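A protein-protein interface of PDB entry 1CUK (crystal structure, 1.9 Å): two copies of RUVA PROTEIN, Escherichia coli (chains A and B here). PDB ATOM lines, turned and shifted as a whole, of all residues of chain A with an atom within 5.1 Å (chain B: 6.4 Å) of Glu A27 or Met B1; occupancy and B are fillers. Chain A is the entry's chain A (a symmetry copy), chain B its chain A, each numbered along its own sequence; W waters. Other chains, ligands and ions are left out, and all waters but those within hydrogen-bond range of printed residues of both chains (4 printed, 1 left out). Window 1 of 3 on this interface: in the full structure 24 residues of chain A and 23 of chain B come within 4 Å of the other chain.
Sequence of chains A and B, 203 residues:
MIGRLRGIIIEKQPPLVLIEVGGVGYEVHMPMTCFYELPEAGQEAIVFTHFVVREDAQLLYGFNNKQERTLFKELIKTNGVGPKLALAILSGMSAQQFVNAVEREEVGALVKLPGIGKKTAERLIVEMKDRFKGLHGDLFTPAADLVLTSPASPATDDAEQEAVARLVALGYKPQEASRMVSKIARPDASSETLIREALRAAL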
ATOM      1  N   ILE A   2       2.851 -20.535 -15.910  1.00  0.00           N
ATOM      2  CA  ILE A   2       3.872 -20.088 -14.910  1.00  0.00           C
ATOM      3  C   ILE A   2       3.251 -19.330 -13.732  1.00  0.00           C
ATOM      4  O   ILE A   2       2.734 -18.241 -13.895  1.00  0.00           O
ATOM      5  CB  ILE A   2       5.026 -19.282 -15.566  1.00  0.00           C
ATOM      6  CG1 ILE A   2       5.679 -20.136 -16.651  1.00  0.00           C
ATOM      7  CG2 ILE A   2       6.113 -18.889 -14.529  1.00  0.00           C
ATOM      8  CD1 ILE A   2       6.581 -19.332 -17.562  1.00  0.00           C
ATOM      9  N   LEU A  16       9.410  -2.661 -14.466  1.00  0.00           N
ATOM     10  CA  LEU A  16       9.928  -3.902 -15.017  1.00  0.00           C
ATOM     11  C   LEU A  16      11.150  -4.416 -14.220  1.00  0.00           C
ATOM     12  O   LEU A  16      12.012  -3.649 -13.790  1.00  0.00           O
ATOM     13  CB  LEU A  16      10.391  -3.561 -16.454  1.00  0.00           C
ATOM     14  CG  LEU A  16      10.375  -4.648 -17.554  1.00  0.00           C
ATOM     15  CD1 LEU A  16      11.504  -5.673 -17.399  1.00  0.00           C
ATOM     16  CD2 LEU A  16       9.006  -5.301 -17.716  1.00  0.00           C
ATOM     17  N   VAL A  17      11.201  -5.707 -14.040  1.00  0.00           N
ATOM     18  CA  VAL A  17      12.331  -6.363 -13.360  1.00  0.00           C
ATOM     19  C   VAL A  17      12.726  -7.551 -14.223  1.00  0.00           C
ATOM     20  O   VAL A  17      11.852  -8.251 -14.732  1.00  0.00           O
ATOM     21  CB  VAL A  17      12.132  -6.735 -11.853  1.00  0.00           C
ATOM     22  CG1 VAL A  17      11.016  -7.782 -11.658  1.00  0.00           C
ATOM     23  CG2 VAL A  17      13.431  -7.313 -11.314  1.00  0.00           C
ATOM     24  N   LEU A  18      14.015  -7.757 -14.421  1.00  0.00           N
ATOM     25  CA  LEU A  18      14.511  -8.857 -15.214  1.00  0.00           C
ATOM     26  C   LEU A  18      15.112  -9.864 -14.248  1.00  0.00           C
ATOM     27  O   LEU A  18      16.066  -9.507 -13.550  1.00  0.00           O
ATOM     28  CB  LEU A  18      15.603  -8.331 -16.148  1.00  0.00           C
ATOM     29  CG  LEU A  18      16.146  -9.361 -17.122  1.00  0.00           C
ATOM     30  CD1 LEU A  18      15.070  -9.831 -18.095  1.00  0.00           C
ATOM     31  CD2 LEU A  18      17.253  -8.687 -17.889  1.00  0.00           C
ATOM     32  N   GLY A  25      16.361 -14.969 -18.992  1.00  0.00           N
ATOM     33  CA  GLY A  25      16.023 -13.730 -18.343  1.00  0.00           C
ATOM     34  C   GLY A  25      14.545 -13.394 -18.600  1.00  0.00           C
ATOM     35  O   GLY A  25      14.160 -13.052 -19.695  1.00  0.00           O
ATOM     36  N   TYR A  26      13.730 -13.521 -17.584  1.00  0.00           N
ATOM     37  CA  TYR A  26      12.295 -13.251 -17.653  1.00  0.00           C
ATOM     38  C   TYR A  26      11.958 -11.829 -17.253  1.00  0.00           C
ATOM     39  O   TYR A  26      12.379 -11.354 -16.212  1.00  0.00           O
ATOM     40  CB  TYR A  26      11.469 -14.169 -16.720  1.00  0.00           C
ATOM     41  CG  TYR A  26      11.389 -15.578 -17.221  1.00  0.00           C
ATOM     42  CD1 TYR A  26      10.412 -15.931 -18.157  1.00  0.00           C
ATOM     43  CD2 TYR A  26      12.291 -16.561 -16.790  1.00  0.00           C
ATOM     44  CE1 TYR A  26      10.319 -17.226 -18.656  1.00  0.00           C
ATOM     45  CE2 TYR A  26      12.210 -17.869 -17.279  1.00  0.00           C
ATOM     46  CZ  TYR A  26      11.221 -18.192 -18.208  1.00  0.00           C
ATOM     47  OH  TYR A  26      11.134 -19.457 -18.692  1.00  0.00           O
ATOM     48  N   GLU A  27      11.170 -11.127 -18.086  1.00  0.00           N
ATOM     49  CA  GLU A  27      10.748  -9.778 -17.753  1.00  0.00           C
ATOM     50  C   GLU A  27       9.492  -9.902 -16.976  1.00  0.00           C
ATOM     51  O   GLU A  27       8.578 -10.622 -17.382  1.00  0.00           O
ATOM     52  CB  GLU A  27      10.356  -8.978 -18.967  1.00  0.00           C
ATOM     53  CG  GLU A  27      11.507  -8.698 -19.886  1.00  0.00           C
ATOM     54  CD  GLU A  27      11.034  -8.070 -21.165  1.00  0.00           C
ATOM     55  OE1 GLU A  27       9.754  -8.327 -21.447  1.00  0.00           O
ATOM     56  OE2 GLU A  27      11.770  -7.416 -21.865  1.00  0.00           O
ATOM     57  N   VAL A  28       9.433  -9.225 -15.858  1.00  0.00           N
ATOM     58  CA  VAL A  28       8.273  -9.275 -14.981  1.00  0.00           C
ATOM     59  C   VAL A  28       7.778  -7.882 -14.715  1.00  0.00           C
ATOM     60  O   VAL A  28       8.571  -7.013 -14.369  1.00  0.00           O
ATOM     61  CB  VAL A  28       8.637  -9.958 -13.662  1.00  0.00           C
ATOM     62  CG1 VAL A  28       7.417 -10.051 -12.779  1.00  0.00           C
ATOM     63  CG2 VAL A  28       9.115 -11.378 -13.944  1.00  0.00           C
ATOM     64  N   HIS A  29       6.461  -7.672 -14.866  1.00  0.00           N
ATOM     65  CA  HIS A  29       5.859  -6.327 -14.623  1.00  0.00           C
ATOM     66  C   HIS A  29       5.264  -6.287 -13.241  1.00  0.00           C
ATOM     67  O   HIS A  29       4.366  -7.078 -12.955  1.00  0.00           O
ATOM     68  CB  HIS A  29       4.786  -5.970 -15.689  1.00  0.00           C
ATOM     69  CG  HIS A  29       5.338  -6.035 -17.078  1.00  0.00           C
ATOM     70  ND1 HIS A  29       5.572  -4.912 -17.808  1.00  0.00           N
ATOM     71  CD2 HIS A  29       5.700  -7.089 -17.837  1.00  0.00           C
ATOM     72  CE1 HIS A  29       6.061  -5.294 -18.981  1.00  0.00           C
ATOM     73  NE2 HIS A  29       6.147  -6.595 -19.037  1.00  0.00           N
ATOM     74  N   PHE A  51       0.206 -14.810 -15.730  1.00  0.00           N
ATOM     75  CA  PHE A  51       0.464 -14.758 -17.131  1.00  0.00           C
ATOM     76  C   PHE A  51      -0.653 -14.115 -17.955  1.00  0.00           C
ATOM     77  O   PHE A  51      -1.823 -14.483 -17.870  1.00  0.00           O
ATOM     78  CB  PHE A  51       0.717 -16.194 -17.611  1.00  0.00           C
ATOM     79  CG  PHE A  51       1.020 -16.367 -19.095  1.00  0.00           C
ATOM     80  CD1 PHE A  51       2.211 -15.873 -19.638  1.00  0.00           C
ATOM     81  CD2 PHE A  51       0.124 -17.046 -19.931  1.00  0.00           C
ATOM     82  CE1 PHE A  51       2.512 -16.027 -20.991  1.00  0.00           C
ATOM     83  CE2 PHE A  51       0.408 -17.210 -21.287  1.00  0.00           C
ATOM     84  CZ  PHE A  51       1.601 -16.700 -21.810  1.00  0.00           C
ATOM     85  N   GLN A  58       3.131 -11.841 -24.847  1.00  0.00           N
ATOM     86  CA  GLN A  58       2.902 -12.718 -23.743  1.00  0.00           C
ATOM     87  C   GLN A  58       3.576 -12.041 -22.557  1.00  0.00           C
ATOM     88  O   GLN A  58       4.732 -11.694 -22.636  1.00  0.00           O
ATOM     89  CB  GLN A  58       3.424 -14.074 -24.024  1.00  0.00           C
ATOM     90  CG  GLN A  58       2.413 -14.794 -24.856  1.00  0.00           C
ATOM     91  CD  GLN A  58       2.944 -16.104 -25.248  1.00  0.00           C
ATOM     92  OE1 GLN A  58       2.312 -16.819 -26.048  1.00  0.00           O
ATOM     93  NE2 GLN A  58       4.121 -16.436 -24.716  1.00  0.00           N
ATOM     94  N   LEU A  59       2.825 -11.775 -21.501  1.00  0.00           N
ATOM     95  CA  LEU A  59       3.408 -11.031 -20.396  1.00  0.00           C
ATOM     96  C   LEU A  59       3.255 -11.700 -19.084  1.00  0.00           C
ATOM     97  O   LEU A  59       2.329 -12.463 -18.892  1.00  0.00           O
ATOM     98  CB  LEU A  59       2.645  -9.712 -20.224  1.00  0.00           C
ATOM     99  CG  LEU A  59       2.697  -8.837 -21.463  1.00  0.00           C
ATOM    100  CD1 LEU A  59       1.902  -7.569 -21.255  1.00  0.00           C
ATOM    101  CD2 LEU A  59       4.141  -8.521 -21.756  1.00  0.00           C
ATOM    102  N   LEU A  60       4.155 -11.330 -18.170  1.00  0.00           N
ATOM    103  CA  LEU A  60       4.090 -11.833 -16.813  1.00  0.00           C
ATOM    104  C   LEU A  60       3.991 -10.660 -15.858  1.00  0.00           C
ATOM    105  O   LEU A  60       4.801  -9.745 -15.886  1.00  0.00           O
ATOM    106  CB  LEU A  60       5.394 -12.624 -16.404  1.00  0.00           C
ATOM    107  CG  LEU A  60       5.554 -14.074 -16.907  1.00  0.00           C
ATOM    108  CD1 LEU A  60       6.922 -14.641 -16.469  1.00  0.00           C
ATOM    109  CD2 LEU A  60       4.386 -14.981 -16.500  1.00  0.00           C
ATOM    110  N   MET B   1       7.706 -12.117 -22.833  1.00  0.00           N
ATOM    111  CA  MET B   1       8.066 -12.648 -21.535  1.00  0.00           C
ATOM    112  C   MET B   1       9.624 -12.734 -21.392  1.00  0.00           C
ATOM    113  O   MET B   1      10.190 -12.366 -20.377  1.00  0.00           O
ATOM    114  CB  MET B   1       7.468 -14.019 -21.486  1.00  0.00           C
ATOM    115  CG  MET B   1       6.966 -14.404 -20.171  1.00  0.00           C
ATOM    116  SD  MET B   1       6.409 -16.109 -20.250  1.00  0.00           S
ATOM    117  CE  MET B   1       6.470 -16.287 -22.038  1.00  0.00           C
ATOM    118  N   ILE B   2      10.292 -13.235 -22.458  1.00  0.00           N
ATOM    119  CA  ILE B   2      11.782 -13.378 -22.503  1.00  0.00           C
ATOM    120  C   ILE B   2      12.483 -12.091 -22.952  1.00  0.00           C
ATOM    121  O   ILE B   2      12.352 -11.673 -24.087  1.00  0.00           O
ATOM    122  CB  ILE B   2      12.232 -14.600 -23.346  1.00  0.00           C
ATOM    123  CG1 ILE B   2      11.593 -15.864 -22.777  1.00  0.00           C
ATOM    124  CG2 ILE B   2      13.776 -14.777 -23.323  1.00  0.00           C
ATOM    125  CD1 ILE B   2      11.700 -17.046 -23.715  1.00  0.00           C
ATOM    126  N   GLY B   3      13.250 -11.475 -22.046  1.00  0.00           N
ATOM    127  CA  GLY B   3      13.980 -10.259 -22.336  1.00  0.00           C
ATOM    128  C   GLY B   3      15.504 -10.489 -22.500  1.00  0.00           C
ATOM    129  O   GLY B   3      16.209  -9.647 -23.024  1.00  0.00           O
ATOM    130  N   ARG B   4      16.039 -11.632 -22.064  1.00  0.00           N
ATOM    131  CA  ARG B   4      17.463 -11.843 -22.217  1.00  0.00           C
ATOM    132  C   ARG B   4      17.835 -13.301 -22.216  1.00  0.00           C
ATOM    133  O   ARG B   4      17.212 -14.093 -21.578  1.00  0.00           O
ATOM    134  CB  ARG B   4      18.254 -11.172 -21.081  1.00  0.00           C
ATOM    135  CG  ARG B   4      19.735 -10.928 -21.453  1.00  0.00           C
ATOM    136  CD  ARG B   4      20.527 -10.387 -20.277  1.00  0.00           C
ATOM    137  NE  ARG B   4      20.906 -11.480 -19.407  1.00  0.00           N
ATOM    138  CZ  ARG B   4      21.888 -11.488 -18.491  1.00  0.00           C
ATOM    139  NH1 ARG B   4      22.656 -10.442 -18.260  1.00  0.00           N
ATOM    140  NH2 ARG B   4      22.098 -12.604 -17.792  1.00  0.00           N
ATOM    141  N   THR B  49      16.571  -9.732 -25.909  1.00  0.00           N
ATOM    142  CA  THR B  49      15.584 -10.166 -26.845  1.00  0.00           C
ATOM    143  C   THR B  49      14.271  -9.447 -26.818  1.00  0.00           C
ATOM    144  O   THR B  49      13.867  -8.875 -25.820  1.00  0.00           O
ATOM    145  CB  THR B  49      15.275 -11.673 -26.654  1.00  0.00           C
ATOM    146  OG1 THR B  49      14.819 -11.882 -25.326  1.00  0.00           O
ATOM    147  CG2 THR B  49      16.507 -12.531 -26.921  1.00  0.00           C
ATOM    148  N   PHE B  51      10.412 -10.463 -28.125  1.00  0.00           N
ATOM    149  CA  PHE B  51       9.552 -11.519 -28.546  1.00  0.00           C
ATOM    150  C   PHE B  51       8.440 -11.082 -29.502  1.00  0.00           C
ATOM    151  O   PHE B  51       7.681 -10.150 -29.240  1.00  0.00           O
ATOM    152  CB  PHE B  51       8.949 -12.158 -27.288  1.00  0.00           C
ATOM    153  CG  PHE B  51       7.991 -13.322 -27.515  1.00  0.00           C
ATOM    154  CD1 PHE B  51       8.460 -14.538 -28.026  1.00  0.00           C
ATOM    155  CD2 PHE B  51       6.634 -13.202 -27.191  1.00  0.00           C
ATOM    156  CE1 PHE B  51       7.603 -15.619 -28.234  1.00  0.00           C
ATOM    157  CE2 PHE B  51       5.762 -14.272 -27.392  1.00  0.00           C
ATOM    158  CZ  PHE B  51       6.251 -15.475 -27.911  1.00  0.00           C
ATOM    159  N   ARG B  69      17.844  -2.541 -28.918  1.00  0.00           N
ATOM    160  CA  ARG B  69      16.530  -3.162 -28.791  1.00  0.00           C
ATOM    161  C   ARG B  69      15.434  -2.093 -28.757  1.00  0.00           C
ATOM    162  O   ARG B  69      14.362  -2.209 -29.373  1.00  0.00           O
ATOM    163  CB  ARG B  69      16.454  -4.049 -27.542  1.00  0.00           C
ATOM    164  CG  ARG B  69      15.197  -4.900 -27.538  1.00  0.00           C
ATOM    165  CD  ARG B  69      15.118  -5.877 -26.370  1.00  0.00           C
ATOM    166  NE  ARG B  69      15.276  -5.200 -25.093  1.00  0.00           N
ATOM    167  CZ  ARG B  69      15.264  -5.822 -23.915  1.00  0.00           C
ATOM    168  NH1 ARG B  69      15.090  -7.144 -23.829  1.00  0.00           N
ATOM    169  NH2 ARG B  69      15.422  -5.094 -22.796  1.00  0.00           N
ATOM    170  N   LYS B  73      12.337  -1.642 -31.119  1.00  0.00           N
ATOM    171  CA  LYS B  73      11.008  -1.557 -30.589  1.00  0.00           C
ATOM    172  C   LYS B  73      10.299  -0.307 -31.114  1.00  0.00           C
ATOM    173  O   LYS B  73       9.143  -0.331 -31.500  1.00  0.00           O
ATOM    174  CB  LYS B  73      11.050  -1.547 -29.087  1.00  0.00           C
ATOM    175  CG  LYS B  73      11.422  -2.922 -28.559  1.00  0.00           C
ATOM    176  CD  LYS B  73      11.167  -3.110 -27.061  1.00  0.00           C
ATOM    177  CE  LYS B  73      11.088  -4.599 -26.698  1.00  0.00           C
ATOM    178  NZ  LYS B  73      11.437  -4.908 -25.313  1.00  0.00           N
HETATM  179  O   HOH W   1      11.761  -7.476 -24.493  1.00  0.00           O
HETATM  180  O   HOH W   2       5.912 -10.487 -25.236  1.00  0.00           O
HETATM  181  O   HOH W   3       9.637 -10.064 -24.081  1.00  0.00           O
HETATM  182  O   HOH W   4      14.832  -6.875 -20.460  1.00  0.00           O
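The backbone carbonyl oxygen (O) of Met B1 lies within hydrogen-bond range of the backbone NH (N) of Glu A27 (2.8 Å). The backbone NH (N) of Met B1 sits at hydrogen-bond distance from the backbone carbonyl oxygen (O) of Gln A58, at 3.0 Å. N of Gly B3 lies within hydrogen-bond range of O of Gly A25 (3.0 Å). The backbone carbonyl oxygen (O) of Arg B4 sits at hydrogen-bond distance from the backbone NH (N) of Gly A25 (2.9 Å). OE2 of Glu A27 lies within salt-bridge range of NH1 of Arg B69 (3.9 Å).
OG1 of Thr B49 lies within hydrogen-bond range of O of Ile B2. The backbone carbonyl oxygen of Gly B3 lies within hydrogen-bond range of the backbone NH of Thr B49, at 2.9 Å. The backbone carbonyl oxygen (O) of Gly B3 lies within hydrogen-bond range of the guanidinium group (NH1) of Arg B69. The backbone NH (N) of Arg B4 sits at hydrogen-bond distance from the side-chain hydroxyl (OG1) of Thr B49, 3.5 Å away. The backbone carbonyl oxygen of Thr B49 sits at hydrogen-bond distance from the guanidinium group of Arg B69 (2.9 Å). The backbone NH (N) of His A29 lies within hydrogen-bond range of the backbone carbonyl oxygen (O) of Leu A60 (2.8 Å).
Among the printed residues, pairs that only touch across the chains: Tyr A26 with Met B1, Leu A60 with Met B1, Glu A27 with Gly B3, Gly A25 with Ile B2, Gln A58 with Phe B51 and Phe A51 with Met B1.
Leu A16 touches none of the printed residues of chain B. Of the printed residues of chain B, Gly A25 touches Ile B2 (3.7 Å), Gly B3 (3.0 Å) and Arg B4 (2.9 Å). Of the printed residues of chain A, Gly B3 touches Gly A25 (3.0 Å) and Glu A27 (3.6 Å). Printed residues of chain A within 4 Å of Arg B4: Gly A25. Of the printed residues of chain A, Phe B51 touches Gln A58. Of the printed residues of chain A, Arg B69 touches Glu A27. The nearest residue of chain B that does not touch Glu A27 is Lys B73 (4.3 Å). The nearest residue of chain A that does not touch Met B1 is Gly A25 (4.1 Å). The nearest printed residue of chain B that does not touch Gly A25 is Met B1 (4.1 Å).
Of the 8 printed residues of chain B, 6 touch a printed residue of chain A. Printed residues of chain B that touch a printed residue of chain A: Met B1, Ile B2, Gly B3, Arg B4, Phe B51 and Arg B69. Of the 13 printed residues of chain A, 6 touch a printed residue of chain B. Printed residues of chain A that touch a printed residue of chain B: Gly A25, Tyr A26, Glu A27, Phe A51, Gln A58 and Leu A60. Hydrophobic or aromatic side chains of chain A within 4 Å of the printed part of chain B: Phe A51 and Leu A60. Among the printed residues, Asp or Glu carboxylates within 4 Å of a Lys or Arg side-chain nitrogen of the other chain: Glu A27 with Arg B69.
Positions printed for both chains: 2 and 51. Of the 11 pairs that touch across the chains among the printed residues, none has its exchanged pair printed and touching as well.
Water W1 lies within hydrogen-bond range of the side-chain carboxylate (OE2) of Glu A27, the side-chain amino group (NZ) of Lys B73, the backbone carbonyl oxygen (O) of Thr B49 and the guanidinium group (NH1) of Arg B69. Water W4 bridges NH2 of Arg B69 and OE2 of Glu A27. Water W3 lies within hydrogen-bond range of N of Met B1, O of Ile B2 and OE1 of Glu A27. Water W2 bridges the backbone carbonyl oxygen of Gln A58 (3.1 Å) and the backbone NH of Met B1 (3.4 Å).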
